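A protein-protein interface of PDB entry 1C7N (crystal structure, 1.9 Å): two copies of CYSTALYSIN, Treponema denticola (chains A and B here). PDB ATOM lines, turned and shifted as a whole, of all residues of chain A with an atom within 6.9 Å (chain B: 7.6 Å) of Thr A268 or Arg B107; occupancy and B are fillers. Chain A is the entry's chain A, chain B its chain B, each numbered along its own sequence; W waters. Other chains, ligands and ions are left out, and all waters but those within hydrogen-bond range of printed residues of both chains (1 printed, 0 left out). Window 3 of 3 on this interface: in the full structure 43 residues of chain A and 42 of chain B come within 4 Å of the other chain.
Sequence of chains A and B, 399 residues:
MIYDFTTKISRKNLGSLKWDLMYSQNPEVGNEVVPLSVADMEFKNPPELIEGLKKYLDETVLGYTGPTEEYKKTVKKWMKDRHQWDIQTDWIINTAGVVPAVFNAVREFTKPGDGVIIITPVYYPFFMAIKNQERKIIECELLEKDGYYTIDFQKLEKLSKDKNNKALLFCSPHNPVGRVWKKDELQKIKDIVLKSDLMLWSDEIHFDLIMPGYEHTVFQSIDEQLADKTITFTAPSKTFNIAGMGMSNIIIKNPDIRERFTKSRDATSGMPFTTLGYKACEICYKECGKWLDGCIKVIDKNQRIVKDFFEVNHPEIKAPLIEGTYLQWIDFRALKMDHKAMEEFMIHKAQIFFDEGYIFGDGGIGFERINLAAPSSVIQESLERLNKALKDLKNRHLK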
ATOM      1  N   PRO A 100     -14.036 -18.114   5.983  1.00  0.00           N
ATOM      2  CA  PRO A 100     -14.903 -17.647   7.071  1.00  0.00           C
ATOM      3  C   PRO A 100     -15.667 -16.386   6.649  1.00  0.00           C
ATOM      4  O   PRO A 100     -16.811 -16.170   7.061  1.00  0.00           O
ATOM      5  CB  PRO A 100     -13.920 -17.378   8.207  1.00  0.00           C
ATOM      6  CG  PRO A 100     -12.864 -18.418   7.976  1.00  0.00           C
ATOM      7  CD  PRO A 100     -12.665 -18.350   6.469  1.00  0.00           C
ATOM      8  N   PHE A 103     -18.577 -17.569   4.530  1.00  0.00           N
ATOM      9  CA  PHE A 103     -19.607 -18.143   5.391  1.00  0.00           C
ATOM     10  C   PHE A 103     -20.388 -17.016   6.047  1.00  0.00           C
ATOM     11  O   PHE A 103     -21.613 -17.087   6.169  1.00  0.00           O
ATOM     12  CB  PHE A 103     -18.985 -19.018   6.484  1.00  0.00           C
ATOM     13  CG  PHE A 103     -18.920 -20.474   6.132  1.00  0.00           C
ATOM     14  CD1 PHE A 103     -17.999 -20.941   5.203  1.00  0.00           C
ATOM     15  CD2 PHE A 103     -19.788 -21.384   6.731  1.00  0.00           C
ATOM     16  CE1 PHE A 103     -17.939 -22.292   4.873  1.00  0.00           C
ATOM     17  CE2 PHE A 103     -19.739 -22.738   6.410  1.00  0.00           C
ATOM     18  CZ  PHE A 103     -18.812 -23.193   5.479  1.00  0.00           C
ATOM     19  N   ASN A 104     -19.668 -15.980   6.471  1.00  0.00           N
ATOM     20  CA  ASN A 104     -20.279 -14.829   7.117  1.00  0.00           C
ATOM     21  C   ASN A 104     -21.191 -14.077   6.151  1.00  0.00           C
ATOM     22  O   ASN A 104     -22.244 -13.577   6.543  1.00  0.00           O
ATOM     23  CB  ASN A 104     -19.198 -13.885   7.645  1.00  0.00           C
ATOM     24  CG  ASN A 104     -19.765 -12.795   8.528  1.00  0.00           C
ATOM     25  OD1 ASN A 104     -20.421 -13.081   9.531  1.00  0.00           O
ATOM     26  ND2 ASN A 104     -19.522 -11.542   8.163  1.00  0.00           N
ATOM     27  N   ARG A 107     -24.361 -16.072   5.875  1.00  0.00           N
ATOM     28  CA  ARG A 107     -25.039 -15.962   7.155  1.00  0.00           C
ATOM     29  C   ARG A 107     -25.813 -14.653   7.306  1.00  0.00           C
ATOM     30  O   ARG A 107     -26.984 -14.652   7.684  1.00  0.00           O
ATOM     31  CB  ARG A 107     -24.009 -16.088   8.282  1.00  0.00           C
ATOM     32  CG  ARG A 107     -24.569 -15.970   9.691  1.00  0.00           C
ATOM     33  CD  ARG A 107     -23.505 -16.314  10.732  1.00  0.00           C
ATOM     34  NE  ARG A 107     -22.883 -17.607  10.451  1.00  0.00           N
ATOM     35  CZ  ARG A 107     -21.664 -17.763   9.938  1.00  0.00           C
ATOM     36  NH1 ARG A 107     -20.914 -16.703   9.649  1.00  0.00           N
ATOM     37  NH2 ARG A 107     -21.198 -18.981   9.699  1.00  0.00           N
ATOM     38  N   LYS A 263     -20.979  -6.691  11.927  1.00  0.00           N
ATOM     39  CA  LYS A 263     -21.783  -7.114  13.073  1.00  0.00           C
ATOM     40  C   LYS A 263     -21.828  -8.636  13.089  1.00  0.00           C
ATOM     41  O   LYS A 263     -21.600  -9.266  14.123  1.00  0.00           O
ATOM     42  CB  LYS A 263     -23.214  -6.570  12.967  1.00  0.00           C
ATOM     43  CG  LYS A 263     -23.955  -7.044  11.722  1.00  0.00           C
ATOM     44  CD  LYS A 263     -25.423  -6.627  11.673  1.00  0.00           C
ATOM     45  CE  LYS A 263     -26.296  -7.538  12.526  1.00  0.00           C
ATOM     46  NZ  LYS A 263     -27.753  -7.294  12.288  1.00  0.00           N
ATOM     47  N   SER A 264     -22.120  -9.224  11.933  1.00  0.00           N
ATOM     48  CA  SER A 264     -22.201 -10.672  11.822  1.00  0.00           C
ATOM     49  C   SER A 264     -20.874 -11.329  12.181  1.00  0.00           C
ATOM     50  O   SER A 264     -20.840 -12.317  12.911  1.00  0.00           O
ATOM     51  CB  SER A 264     -22.609 -11.078  10.408  1.00  0.00           C
ATOM     52  OG  SER A 264     -22.742 -12.485  10.327  1.00  0.00           O
ATOM     53  N   ARG A 265     -19.780 -10.781  11.665  1.00  0.00           N
ATOM     54  CA  ARG A 265     -18.465 -11.323  11.972  1.00  0.00           C
ATOM     55  C   ARG A 265     -18.211 -11.255  13.479  1.00  0.00           C
ATOM     56  O   ARG A 265     -17.660 -12.187  14.067  1.00  0.00           O
ATOM     57  CB  ARG A 265     -17.373 -10.544  11.229  1.00  0.00           C
ATOM     58  CG  ARG A 265     -15.981 -10.755  11.799  1.00  0.00           C
ATOM     59  CD  ARG A 265     -15.572  -9.563  12.648  1.00  0.00           C
ATOM     60  NE  ARG A 265     -14.629  -8.734  11.920  1.00  0.00           N
ATOM     61  CZ  ARG A 265     -14.205  -7.536  12.306  1.00  0.00           C
ATOM     62  NH1 ARG A 265     -14.643  -6.985  13.431  1.00  0.00           N
ATOM     63  NH2 ARG A 265     -13.321  -6.893  11.564  1.00  0.00           N
ATOM     64  N   ASP A 266     -18.635 -10.162  14.104  1.00  0.00           N
ATOM     65  CA  ASP A 266     -18.422  -9.990  15.537  1.00  0.00           C
ATOM     66  C   ASP A 266     -19.227 -10.950  16.411  1.00  0.00           C
ATOM     67  O   ASP A 266     -18.951 -11.077  17.605  1.00  0.00           O
ATOM     68  CB  ASP A 266     -18.700  -8.540  15.947  1.00  0.00           C
ATOM     69  CG  ASP A 266     -17.709  -7.562  15.335  1.00  0.00           C
ATOM     70  OD1 ASP A 266     -16.529  -7.938  15.164  1.00  0.00           O
ATOM     71  OD2 ASP A 266     -18.100  -6.416  15.035  1.00  0.00           O
ATOM     72  N   ALA A 267     -20.216 -11.617  15.824  1.00  0.00           N
ATOM     73  CA  ALA A 267     -21.026 -12.582  16.562  1.00  0.00           C
ATOM     74  C   ALA A 267     -20.465 -13.979  16.312  1.00  0.00           C
ATOM     75  O   ALA A 267     -20.746 -14.915  17.059  1.00  0.00           O
ATOM     76  CB  ALA A 267     -22.483 -12.513  16.112  1.00  0.00           C
ATOM     77  N   THR A 268     -19.676 -14.105  15.248  1.00  0.00           N
ATOM     78  CA  THR A 268     -19.044 -15.368  14.870  1.00  0.00           C
ATOM     79  C   THR A 268     -17.618 -15.067  14.409  1.00  0.00           C
ATOM     80  O   THR A 268     -17.424 -14.426  13.377  1.00  0.00           O
ATOM     81  CB  THR A 268     -19.775 -16.047  13.693  1.00  0.00           C
ATOM     82  OG1 THR A 268     -19.480 -15.345  12.482  1.00  0.00           O
ATOM     83  CG2 THR A 268     -21.283 -16.030  13.914  1.00  0.00           C
ATOM     84  N   SER A 269     -16.638 -15.531  15.176  1.00  0.00           N
ATOM     85  CA  SER A 269     -15.218 -15.322  14.879  1.00  0.00           C
ATOM     86  C   SER A 269     -14.692 -14.087  15.593  1.00  0.00           C
ATOM     87  O   SER A 269     -13.647 -14.130  16.243  1.00  0.00           O
ATOM     88  CB  SER A 269     -14.975 -15.158  13.370  1.00  0.00           C
ATOM     89  OG  SER A 269     -15.504 -16.244  12.624  1.00  0.00           O
ATOM     90  N   GLY A 270     -15.423 -12.986  15.473  1.00  0.00           N
ATOM     91  CA  GLY A 270     -14.987 -11.752  16.093  1.00  0.00           C
ATOM     92  C   GLY A 270     -13.854 -11.134  15.293  1.00  0.00           C
ATOM     93  O   GLY A 270     -13.453 -11.661  14.254  1.00  0.00           O
ATOM     94  N   MET A 271     -13.335 -10.015  15.781  1.00  0.00           N
ATOM     95  CA  MET A 271     -12.246  -9.299  15.125  1.00  0.00           C
ATOM     96  C   MET A 271     -10.914 -10.033  15.298  1.00  0.00           C
ATOM     97  O   MET A 271     -10.625 -10.550  16.375  1.00  0.00           O
ATOM     98  CB  MET A 271     -12.141  -7.897  15.732  1.00  0.00           C
ATOM     99  CG  MET A 271     -11.055  -7.012  15.148  1.00  0.00           C
ATOM    100  SD  MET A 271     -10.757  -5.562  16.204  1.00  0.00           S
ATOM    101  CE  MET A 271      -8.964  -5.560  16.279  1.00  0.00           C
ATOM    102  N   VAL B  99     -13.276 -15.946  23.576  1.00  0.00           N
ATOM    103  CA  VAL B  99     -14.560 -15.310  23.330  1.00  0.00           C
ATOM    104  C   VAL B  99     -15.305 -16.016  22.192  1.00  0.00           C
ATOM    105  O   VAL B  99     -16.489 -16.328  22.321  1.00  0.00           O
ATOM    106  CB  VAL B  99     -14.388 -13.809  23.035  1.00  0.00           C
ATOM    107  CG1 VAL B  99     -15.733 -13.183  22.662  1.00  0.00           C
ATOM    108  CG2 VAL B  99     -13.830 -13.122  24.276  1.00  0.00           C
ATOM    109  N   PRO B 100     -14.629 -16.279  21.063  1.00  0.00           N
ATOM    110  CA  PRO B 100     -15.332 -16.964  19.974  1.00  0.00           C
ATOM    111  C   PRO B 100     -15.848 -18.330  20.430  1.00  0.00           C
ATOM    112  O   PRO B 100     -16.907 -18.786  19.993  1.00  0.00           O
ATOM    113  CB  PRO B 100     -14.264 -17.076  18.892  1.00  0.00           C
ATOM    114  CG  PRO B 100     -13.453 -15.834  19.106  1.00  0.00           C
ATOM    115  CD  PRO B 100     -13.306 -15.805  20.617  1.00  0.00           C
ATOM    116  N   ALA B 101     -15.093 -18.989  21.308  1.00  0.00           N
ATOM    117  CA  ALA B 101     -15.503 -20.295  21.815  1.00  0.00           C
ATOM    118  C   ALA B 101     -16.797 -20.151  22.620  1.00  0.00           C
ATOM    119  O   ALA B 101     -17.683 -21.005  22.545  1.00  0.00           O
ATOM    120  CB  ALA B 101     -14.400 -20.898  22.686  1.00  0.00           C
ATOM    121  N   VAL B 102     -16.905 -19.069  23.386  1.00  0.00           N
ATOM    122  CA  VAL B 102     -18.107 -18.837  24.174  1.00  0.00           C
ATOM    123  C   VAL B 102     -19.291 -18.583  23.249  1.00  0.00           C
ATOM    124  O   VAL B 102     -20.389 -19.086  23.490  1.00  0.00           O
ATOM    125  CB  VAL B 102     -17.960 -17.626  25.116  1.00  0.00           C
ATOM    126  CG1 VAL B 102     -19.272 -17.400  25.870  1.00  0.00           C
ATOM    127  CG2 VAL B 102     -16.822 -17.863  26.097  1.00  0.00           C
ATOM    128  N   PHE B 103     -19.079 -17.788  22.201  1.00  0.00           N
ATOM    129  CA  PHE B 103     -20.157 -17.504  21.257  1.00  0.00           C
ATOM    130  C   PHE B 103     -20.604 -18.822  20.649  1.00  0.00           C
ATOM    131  O   PHE B 103     -21.794 -19.053  20.426  1.00  0.00           O
ATOM    132  CB  PHE B 103     -19.687 -16.572  20.133  1.00  0.00           C
ATOM    133  CG  PHE B 103     -19.858 -15.115  20.440  1.00  0.00           C
ATOM    134  CD1 PHE B 103     -19.037 -14.482  21.366  1.00  0.00           C
ATOM    135  CD2 PHE B 103     -20.849 -14.373  19.802  1.00  0.00           C
ATOM    136  CE1 PHE B 103     -19.199 -13.126  21.652  1.00  0.00           C
ATOM    137  CE2 PHE B 103     -21.021 -13.018  20.079  1.00  0.00           C
ATOM    138  CZ  PHE B 103     -20.193 -12.393  21.008  1.00  0.00           C
ATOM    139  N   ASN B 104     -19.626 -19.681  20.391  1.00  0.00           N
ATOM    140  CA  ASN B 104     -19.863 -20.992  19.811  1.00  0.00           C
ATOM    141  C   ASN B 104     -20.728 -21.852  20.721  1.00  0.00           C
ATOM    142  O   ASN B 104     -21.648 -22.532  20.257  1.00  0.00           O
ATOM    143  CB  ASN B 104     -18.525 -21.683  19.570  1.00  0.00           C
ATOM    144  CG  ASN B 104     -18.362 -22.144  18.148  1.00  0.00           C
ATOM    145  OD1 ASN B 104     -17.236 -22.327  17.669  1.00  0.00           O
ATOM    146  ND2 ASN B 104     -19.480 -22.346  17.458  1.00  0.00           N
ATOM    147  N   ALA B 105     -20.425 -21.826  22.017  1.00  0.00           N
ATOM    148  CA  ALA B 105     -21.176 -22.608  22.995  1.00  0.00           C
ATOM    149  C   ALA B 105     -22.630 -22.150  23.031  1.00  0.00           C
ATOM    150  O   ALA B 105     -23.551 -22.965  23.001  1.00  0.00           O
ATOM    151  CB  ALA B 105     -20.550 -22.455  24.381  1.00  0.00           C
ATOM    152  N   VAL B 106     -22.823 -20.836  23.091  1.00  0.00           N
ATOM    153  CA  VAL B 106     -24.157 -20.247  23.130  1.00  0.00           C
ATOM    154  C   VAL B 106     -24.942 -20.596  21.868  1.00  0.00           C
ATOM    155  O   VAL B 106     -26.114 -20.960  21.934  1.00  0.00           O
ATOM    156  CB  VAL B 106     -24.073 -18.709  23.263  1.00  0.00           C
ATOM    157  CG1 VAL B 106     -25.449 -18.080  23.084  1.00  0.00           C
ATOM    158  CG2 VAL B 106     -23.500 -18.345  24.627  1.00  0.00           C
ATOM    159  N   ARG B 107     -24.291 -20.496  20.717  1.00  0.00           N
ATOM    160  CA  ARG B 107     -24.958 -20.784  19.453  1.00  0.00           C
ATOM    161  C   ARG B 107     -25.339 -22.249  19.253  1.00  0.00           C
ATOM    162  O   ARG B 107     -26.369 -22.553  18.650  1.00  0.00           O
ATOM    163  CB  ARG B 107     -24.081 -20.314  18.289  1.00  0.00           C
ATOM    164  CG  ARG B 107     -24.604 -20.694  16.916  1.00  0.00           C
ATOM    165  CD  ARG B 107     -23.910 -19.902  15.815  1.00  0.00           C
ATOM    166  NE  ARG B 107     -22.459 -19.879  15.974  1.00  0.00           N
ATOM    167  CZ  ARG B 107     -21.763 -18.810  16.348  1.00  0.00           C
ATOM    168  NH1 ARG B 107     -22.382 -17.664  16.602  1.00  0.00           N
ATOM    169  NH2 ARG B 107     -20.444 -18.889  16.470  1.00  0.00           N
ATOM    170  N   GLU B 108     -24.521 -23.160  19.769  1.00  0.00           N
ATOM    171  CA  GLU B 108     -24.779 -24.581  19.589  1.00  0.00           C
ATOM    172  C   GLU B 108     -25.595 -25.278  20.673  1.00  0.00           C
ATOM    173  O   GLU B 108     -26.351 -26.206  20.376  1.00  0.00           O
ATOM    174  CB  GLU B 108     -23.450 -25.314  19.412  1.00  0.00           C
ATOM    175  CG  GLU B 108     -23.563 -26.824  19.334  1.00  0.00           C
ATOM    176  CD  GLU B 108     -24.465 -27.291  18.208  1.00  0.00           C
ATOM    177  OE1 GLU B 108     -24.438 -26.674  17.124  1.00  0.00           O
ATOM    178  OE2 GLU B 108     -25.188 -28.289  18.403  1.00  0.00           O
ATOM    179  N   PHE B 109     -25.456 -24.848  21.923  1.00  0.00           N
ATOM    180  CA  PHE B 109     -26.181 -25.510  23.004  1.00  0.00           C
ATOM    181  C   PHE B 109     -27.397 -24.802  23.596  1.00  0.00           C
ATOM    182  O   PHE B 109     -27.905 -25.197  24.646  1.00  0.00           O
ATOM    183  CB  PHE B 109     -25.199 -25.888  24.113  1.00  0.00           C
ATOM    184  CG  PHE B 109     -24.105 -26.800  23.645  1.00  0.00           C
ATOM    185  CD1 PHE B 109     -22.882 -26.283  23.224  1.00  0.00           C
ATOM    186  CD2 PHE B 109     -24.316 -28.176  23.570  1.00  0.00           C
ATOM    187  CE1 PHE B 109     -21.883 -27.127  22.728  1.00  0.00           C
ATOM    188  CE2 PHE B 109     -23.321 -29.029  23.075  1.00  0.00           C
ATOM    189  CZ  PHE B 109     -22.104 -28.504  22.654  1.00  0.00           C
ATOM    190  N   THR B 110     -27.862 -23.757  22.920  1.00  0.00           N
ATOM    191  CA  THR B 110     -29.037 -23.015  23.358  1.00  0.00           C
ATOM    192  C   THR B 110     -29.714 -22.477  22.108  1.00  0.00           C
ATOM    193  O   THR B 110     -29.131 -22.492  21.027  1.00  0.00           O
ATOM    194  CB  THR B 110     -28.673 -21.805  24.255  1.00  0.00           C
ATOM    195  OG1 THR B 110     -27.984 -20.822  23.475  1.00  0.00           O
ATOM    196  CG2 THR B 110     -27.797 -22.234  25.416  1.00  0.00           C
ATOM    197  N   LYS B 111     -30.949 -22.017  22.254  1.00  0.00           N
ATOM    198  CA  LYS B 111     -31.675 -21.446  21.130  1.00  0.00           C
ATOM    199  C   LYS B 111     -32.199 -20.075  21.524  1.00  0.00           C
ATOM    200  O   LYS B 111     -32.244 -19.738  22.710  1.00  0.00           O
ATOM    201  CB  LYS B 111     -32.824 -22.367  20.684  1.00  0.00           C
ATOM    202  CG  LYS B 111     -33.280 -23.404  21.705  1.00  0.00           C
ATOM    203  CD  LYS B 111     -34.432 -22.912  22.570  1.00  0.00           C
ATOM    204  CE  LYS B 111     -34.923 -24.027  23.490  1.00  0.00           C
ATOM    205  NZ  LYS B 111     -35.976 -23.609  24.456  1.00  0.00           N
ATOM    206  N   PRO B 112     -32.574 -19.248  20.532  1.00  0.00           N
ATOM    207  CA  PRO B 112     -33.087 -17.912  20.844  1.00  0.00           C
ATOM    208  C   PRO B 112     -34.125 -17.976  21.964  1.00  0.00           C
ATOM    209  O   PRO B 112     -34.985 -18.858  21.975  1.00  0.00           O
ATOM    210  CB  PRO B 112     -33.681 -17.458  19.516  1.00  0.00           C
ATOM    211  CG  PRO B 112     -32.771 -18.106  18.515  1.00  0.00           C
ATOM    212  CD  PRO B 112     -32.597 -19.499  19.080  1.00  0.00           C
ATOM    213  N   ALA B 129     -21.920 -12.150  24.241  1.00  0.00           N
ATOM    214  CA  ALA B 129     -22.040 -13.491  23.672  1.00  0.00           C
ATOM    215  C   ALA B 129     -23.465 -14.030  23.762  1.00  0.00           C
ATOM    216  O   ALA B 129     -23.941 -14.722  22.856  1.00  0.00           O
ATOM    217  CB  ALA B 129     -21.078 -14.442  24.375  1.00  0.00           C
ATOM    218  N   GLN B 133     -26.936 -12.722  20.551  1.00  0.00           N
ATOM    219  CA  GLN B 133     -27.355 -13.897  19.805  1.00  0.00           C
ATOM    220  C   GLN B 133     -28.821 -14.201  20.106  1.00  0.00           C
ATOM    221  O   GLN B 133     -29.330 -15.273  19.780  1.00  0.00           O
ATOM    222  CB  GLN B 133     -26.464 -15.098  20.136  1.00  0.00           C
ATOM    223  CG  GLN B 133     -25.001 -14.884  19.753  1.00  0.00           C
ATOM    224  CD  GLN B 133     -24.212 -16.178  19.667  1.00  0.00           C
ATOM    225  OE1 GLN B 133     -24.465 -17.016  18.801  1.00  0.00           O
ATOM    226  NE2 GLN B 133     -23.252 -16.347  20.567  1.00  0.00           N
ATOM    227  N   ARG B 135     -30.261 -14.480  23.091  1.00  0.00           N
ATOM    228  CA  ARG B 135     -30.433 -15.360  24.238  1.00  0.00           C
ATOM    229  C   ARG B 135     -30.631 -14.438  25.434  1.00  0.00           C
ATOM    230  O   ARG B 135     -30.286 -13.260  25.371  1.00  0.00           O
ATOM    231  CB  ARG B 135     -29.198 -16.239  24.450  1.00  0.00           C
ATOM    232  CG  ARG B 135     -29.223 -17.572  23.707  1.00  0.00           C
ATOM    233  CD  ARG B 135     -29.160 -17.413  22.190  1.00  0.00           C
ATOM    234  NE  ARG B 135     -28.962 -18.705  21.538  1.00  0.00           N
ATOM    235  CZ  ARG B 135     -28.895 -18.890  20.224  1.00  0.00           C
ATOM    236  NH1 ARG B 135     -29.015 -17.863  19.391  1.00  0.00           N
ATOM    237  NH2 ARG B 135     -28.692 -20.107  19.738  1.00  0.00           N
ATOM    238  N   TRP B 201     -20.083 -24.054  31.590  1.00  0.00           N
ATOM    239  CA  TRP B 201     -19.080 -23.509  30.677  1.00  0.00           C
ATOM    240  C   TRP B 201     -18.137 -22.726  31.563  1.00  0.00           C
ATOM    241  O   TRP B 201     -18.423 -21.587  31.934  1.00  0.00           O
ATOM    242  CB  TRP B 201     -19.711 -22.567  29.649  1.00  0.00           C
ATOM    243  CG  TRP B 201     -20.796 -23.186  28.840  1.00  0.00           C
ATOM    244  CD1 TRP B 201     -21.018 -24.522  28.642  1.00  0.00           C
ATOM    245  CD2 TRP B 201     -21.809 -22.496  28.106  1.00  0.00           C
ATOM    246  NE1 TRP B 201     -22.113 -24.705  27.832  1.00  0.00           N
ATOM    247  CE2 TRP B 201     -22.619 -23.476  27.488  1.00  0.00           C
ATOM    248  CE3 TRP B 201     -22.116 -21.144  27.910  1.00  0.00           C
ATOM    249  CZ2 TRP B 201     -23.716 -23.146  26.685  1.00  0.00           C
ATOM    250  CZ3 TRP B 201     -23.205 -20.815  27.110  1.00  0.00           C
ATOM    251  CH2 TRP B 201     -23.991 -21.814  26.508  1.00  0.00           C
ATOM    252  N   ARG B 260     -20.425 -31.736  18.724  1.00  0.00           N
ATOM    253  CA  ARG B 260     -21.342 -30.640  18.423  1.00  0.00           C
ATOM    254  C   ARG B 260     -20.612 -29.293  18.426  1.00  0.00           C
ATOM    255  O   ARG B 260     -20.804 -28.468  17.533  1.00  0.00           O
ATOM    256  CB  ARG B 260     -22.492 -30.617  19.437  1.00  0.00           C
ATOM    257  CG  ARG B 260     -23.509 -31.751  19.252  1.00  0.00           C
ATOM    258  CD  ARG B 260     -24.606 -31.714  20.322  1.00  0.00           C
ATOM    259  NE  ARG B 260     -25.355 -30.460  20.305  1.00  0.00           N
ATOM    260  CZ  ARG B 260     -26.267 -30.120  21.210  1.00  0.00           C
ATOM    261  NH1 ARG B 260     -26.553 -30.937  22.213  1.00  0.00           N
ATOM    262  NH2 ARG B 260     -26.894 -28.955  21.115  1.00  0.00           N
ATOM    263  N   SER B 264     -20.208 -26.747  15.273  1.00  0.00           N
ATOM    264  CA  SER B 264     -20.626 -25.351  15.326  1.00  0.00           C
ATOM    265  C   SER B 264     -19.468 -24.445  14.928  1.00  0.00           C
ATOM    266  O   SER B 264     -19.653 -23.456  14.222  1.00  0.00           O
ATOM    267  CB  SER B 264     -21.105 -24.991  16.734  1.00  0.00           C
ATOM    268  OG  SER B 264     -21.720 -23.712  16.756  1.00  0.00           O
ATOM    269  N   ARG B 265     -18.270 -24.789  15.386  1.00  0.00           N
ATOM    270  CA  ARG B 265     -17.087 -24.002  15.062  1.00  0.00           C
ATOM    271  C   ARG B 265     -16.831 -24.018  13.559  1.00  0.00           C
ATOM    272  O   ARG B 265     -16.580 -22.983  12.942  1.00  0.00           O
ATOM    273  CB  ARG B 265     -15.851 -24.568  15.765  1.00  0.00           C
ATOM    274  CG  ARG B 265     -14.581 -23.800  15.440  1.00  0.00           C
ATOM    275  CD  ARG B 265     -13.339 -24.623  15.718  1.00  0.00           C
ATOM    276  NE  ARG B 265     -13.243 -25.782  14.833  1.00  0.00           N
ATOM    277  CZ  ARG B 265     -12.291 -26.704  14.917  1.00  0.00           C
ATOM    278  NH1 ARG B 265     -11.350 -26.603  15.846  1.00  0.00           N
ATOM    279  NH2 ARG B 265     -12.285 -27.737  14.084  1.00  0.00           N
ATOM    280  N   ALA B 267     -18.811 -24.339  11.136  1.00  0.00           N
ATOM    281  CA  ALA B 267     -19.817 -23.662  10.324  1.00  0.00           C
ATOM    282  C   ALA B 267     -19.702 -22.145  10.448  1.00  0.00           C
ATOM    283  O   ALA B 267     -20.381 -21.404   9.740  1.00  0.00           O
ATOM    284  CB  ALA B 267     -21.217 -24.114  10.736  1.00  0.00           C
ATOM    285  N   THR B 268     -18.836 -21.683  11.341  1.00  0.00           N
ATOM    286  CA  THR B 268     -18.669 -20.252  11.539  1.00  0.00           C
ATOM    287  C   THR B 268     -17.251 -19.742  11.300  1.00  0.00           C
ATOM    288  O   THR B 268     -17.025 -18.916  10.411  1.00  0.00           O
ATOM    289  CB  THR B 268     -19.114 -19.839  12.957  1.00  0.00           C
ATOM    290  OG1 THR B 268     -18.404 -20.615  13.931  1.00  0.00           O
ATOM    291  CG2 THR B 268     -20.614 -20.068  13.134  1.00  0.00           C
ATOM    292  N   SER B 269     -16.296 -20.231  12.085  1.00  0.00           N
ATOM    293  CA  SER B 269     -14.910 -19.787  11.954  1.00  0.00           C
ATOM    294  C   SER B 269     -13.975 -20.820  11.336  1.00  0.00           C
ATOM    295  O   SER B 269     -12.891 -20.480  10.854  1.00  0.00           O
ATOM    296  CB  SER B 269     -14.363 -19.391  13.329  1.00  0.00           C
ATOM    297  OG  SER B 269     -15.179 -18.409  13.945  1.00  0.00           O
HETATM  298  O   HOH W   1     -12.715 -16.951  15.803  1.00  0.00           O
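NH1 of Arg A107 sits at hydrogen-bond distance from OG1 of Thr A268. OG1 of Thr A268 lies within hydrogen-bond range of O of Ser A264. The guanidinium group of Arg A265 is in salt-bridge range of the side-chain carboxylate of Asp A266 (2.7 Å). The side-chain amide nitrogen (NE2) of Gln B133 lies within hydrogen-bond range of the backbone carbonyl oxygen (O) of Phe B103, at 3.1 Å. OE1 of Gln B133 sits at hydrogen-bond distance from NH1 of Arg B107 (3.1 Å). O of Ser B264 lies within hydrogen-bond range of OG1 of Thr B268 (3.1 Å).
Water W1 bridges O of Ser A269 (3.0 Å) and OG of Ser B269 (3.4 Å).
Hydrophobic or aromatic side chains of chain A that line the printed part of chain B: Pro A100 and Phe A103. Among the printed residues, 12 pairs touch across the chains. Among the printed residues, no Asp or Glu carboxylate lies within 4 Å of a Lys or Arg side-chain nitrogen of the other chain.
Printed residues of chain B within 4 Å of Pro A100: Ser B269. Of chain B, only Phe B103 (2.8 Å) and Arg B107 (3.2 Å) come within 4 Å of Ala A267. Thr A268 touches two residues of chain B. Printed residues of chain A within 4 Å of Phe B103: Asp A266 (3.8 Å) and Ala A267 (2.8 Å). Arg B107 touches just these residues of chain A: Ala A267 and Thr A268. Pro B112 touches none of the printed residues of chain A. Trp B201 touches none of the printed residues of chain A. Of the printed residues of chain A, Thr B268 touches Arg A107 (3.4 Å), Thr A268 (3.9 Å) and Ser A269 (3.8 Å). The nearest residue of chain A that does not touch Arg B107 is Ser A269 (5.2 Å). The nearest printed residue of chain A that does not touch Pro B100 is Gly A270 (5.0 Å).
NH2 of Arg A107 lies within hydrogen-bond range of O of Ala B267. O of Ala A267 lies within hydrogen-bond range of NH1 of Arg B107, 3.2 Å away. The side-chain hydroxyl of Ser B269 lies within hydrogen-bond range of the side-chain hydroxyl of Ser A269 (2.6 Å).
Phe A103 touches Ala B267, and with the chains exchanged Ala A267 touches Phe B103. Arg A107 touches Ala B267, and with the chains exchanged Ala A267 touches Arg B107. Arg A107 touches Thr B268, and with the chains exchanged Thr A268 touches Arg B107. Ser A269 touches Thr B268, but with the chains exchanged Thr A268 does not touch Ser B269 (4.2 Å). 9 positions are printed for both chains.
Pro A100 touches Ser B269. CD2 of Phe A103 touches O of Ala B267, at 3.1 Å. Arg A107 touches Thr B268 (NH2 to CA, 3.4 Å). Phe B103 touches Asp A266. Phe B103 touches Ala A267. Thr A268 touches Arg B107. CB of Thr B268 touches CB of Thr A268, at 3.9 Å. Ser A269 touches Pro B100. OG of Ser A269 touches O of Thr B268 (3.8 Å).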
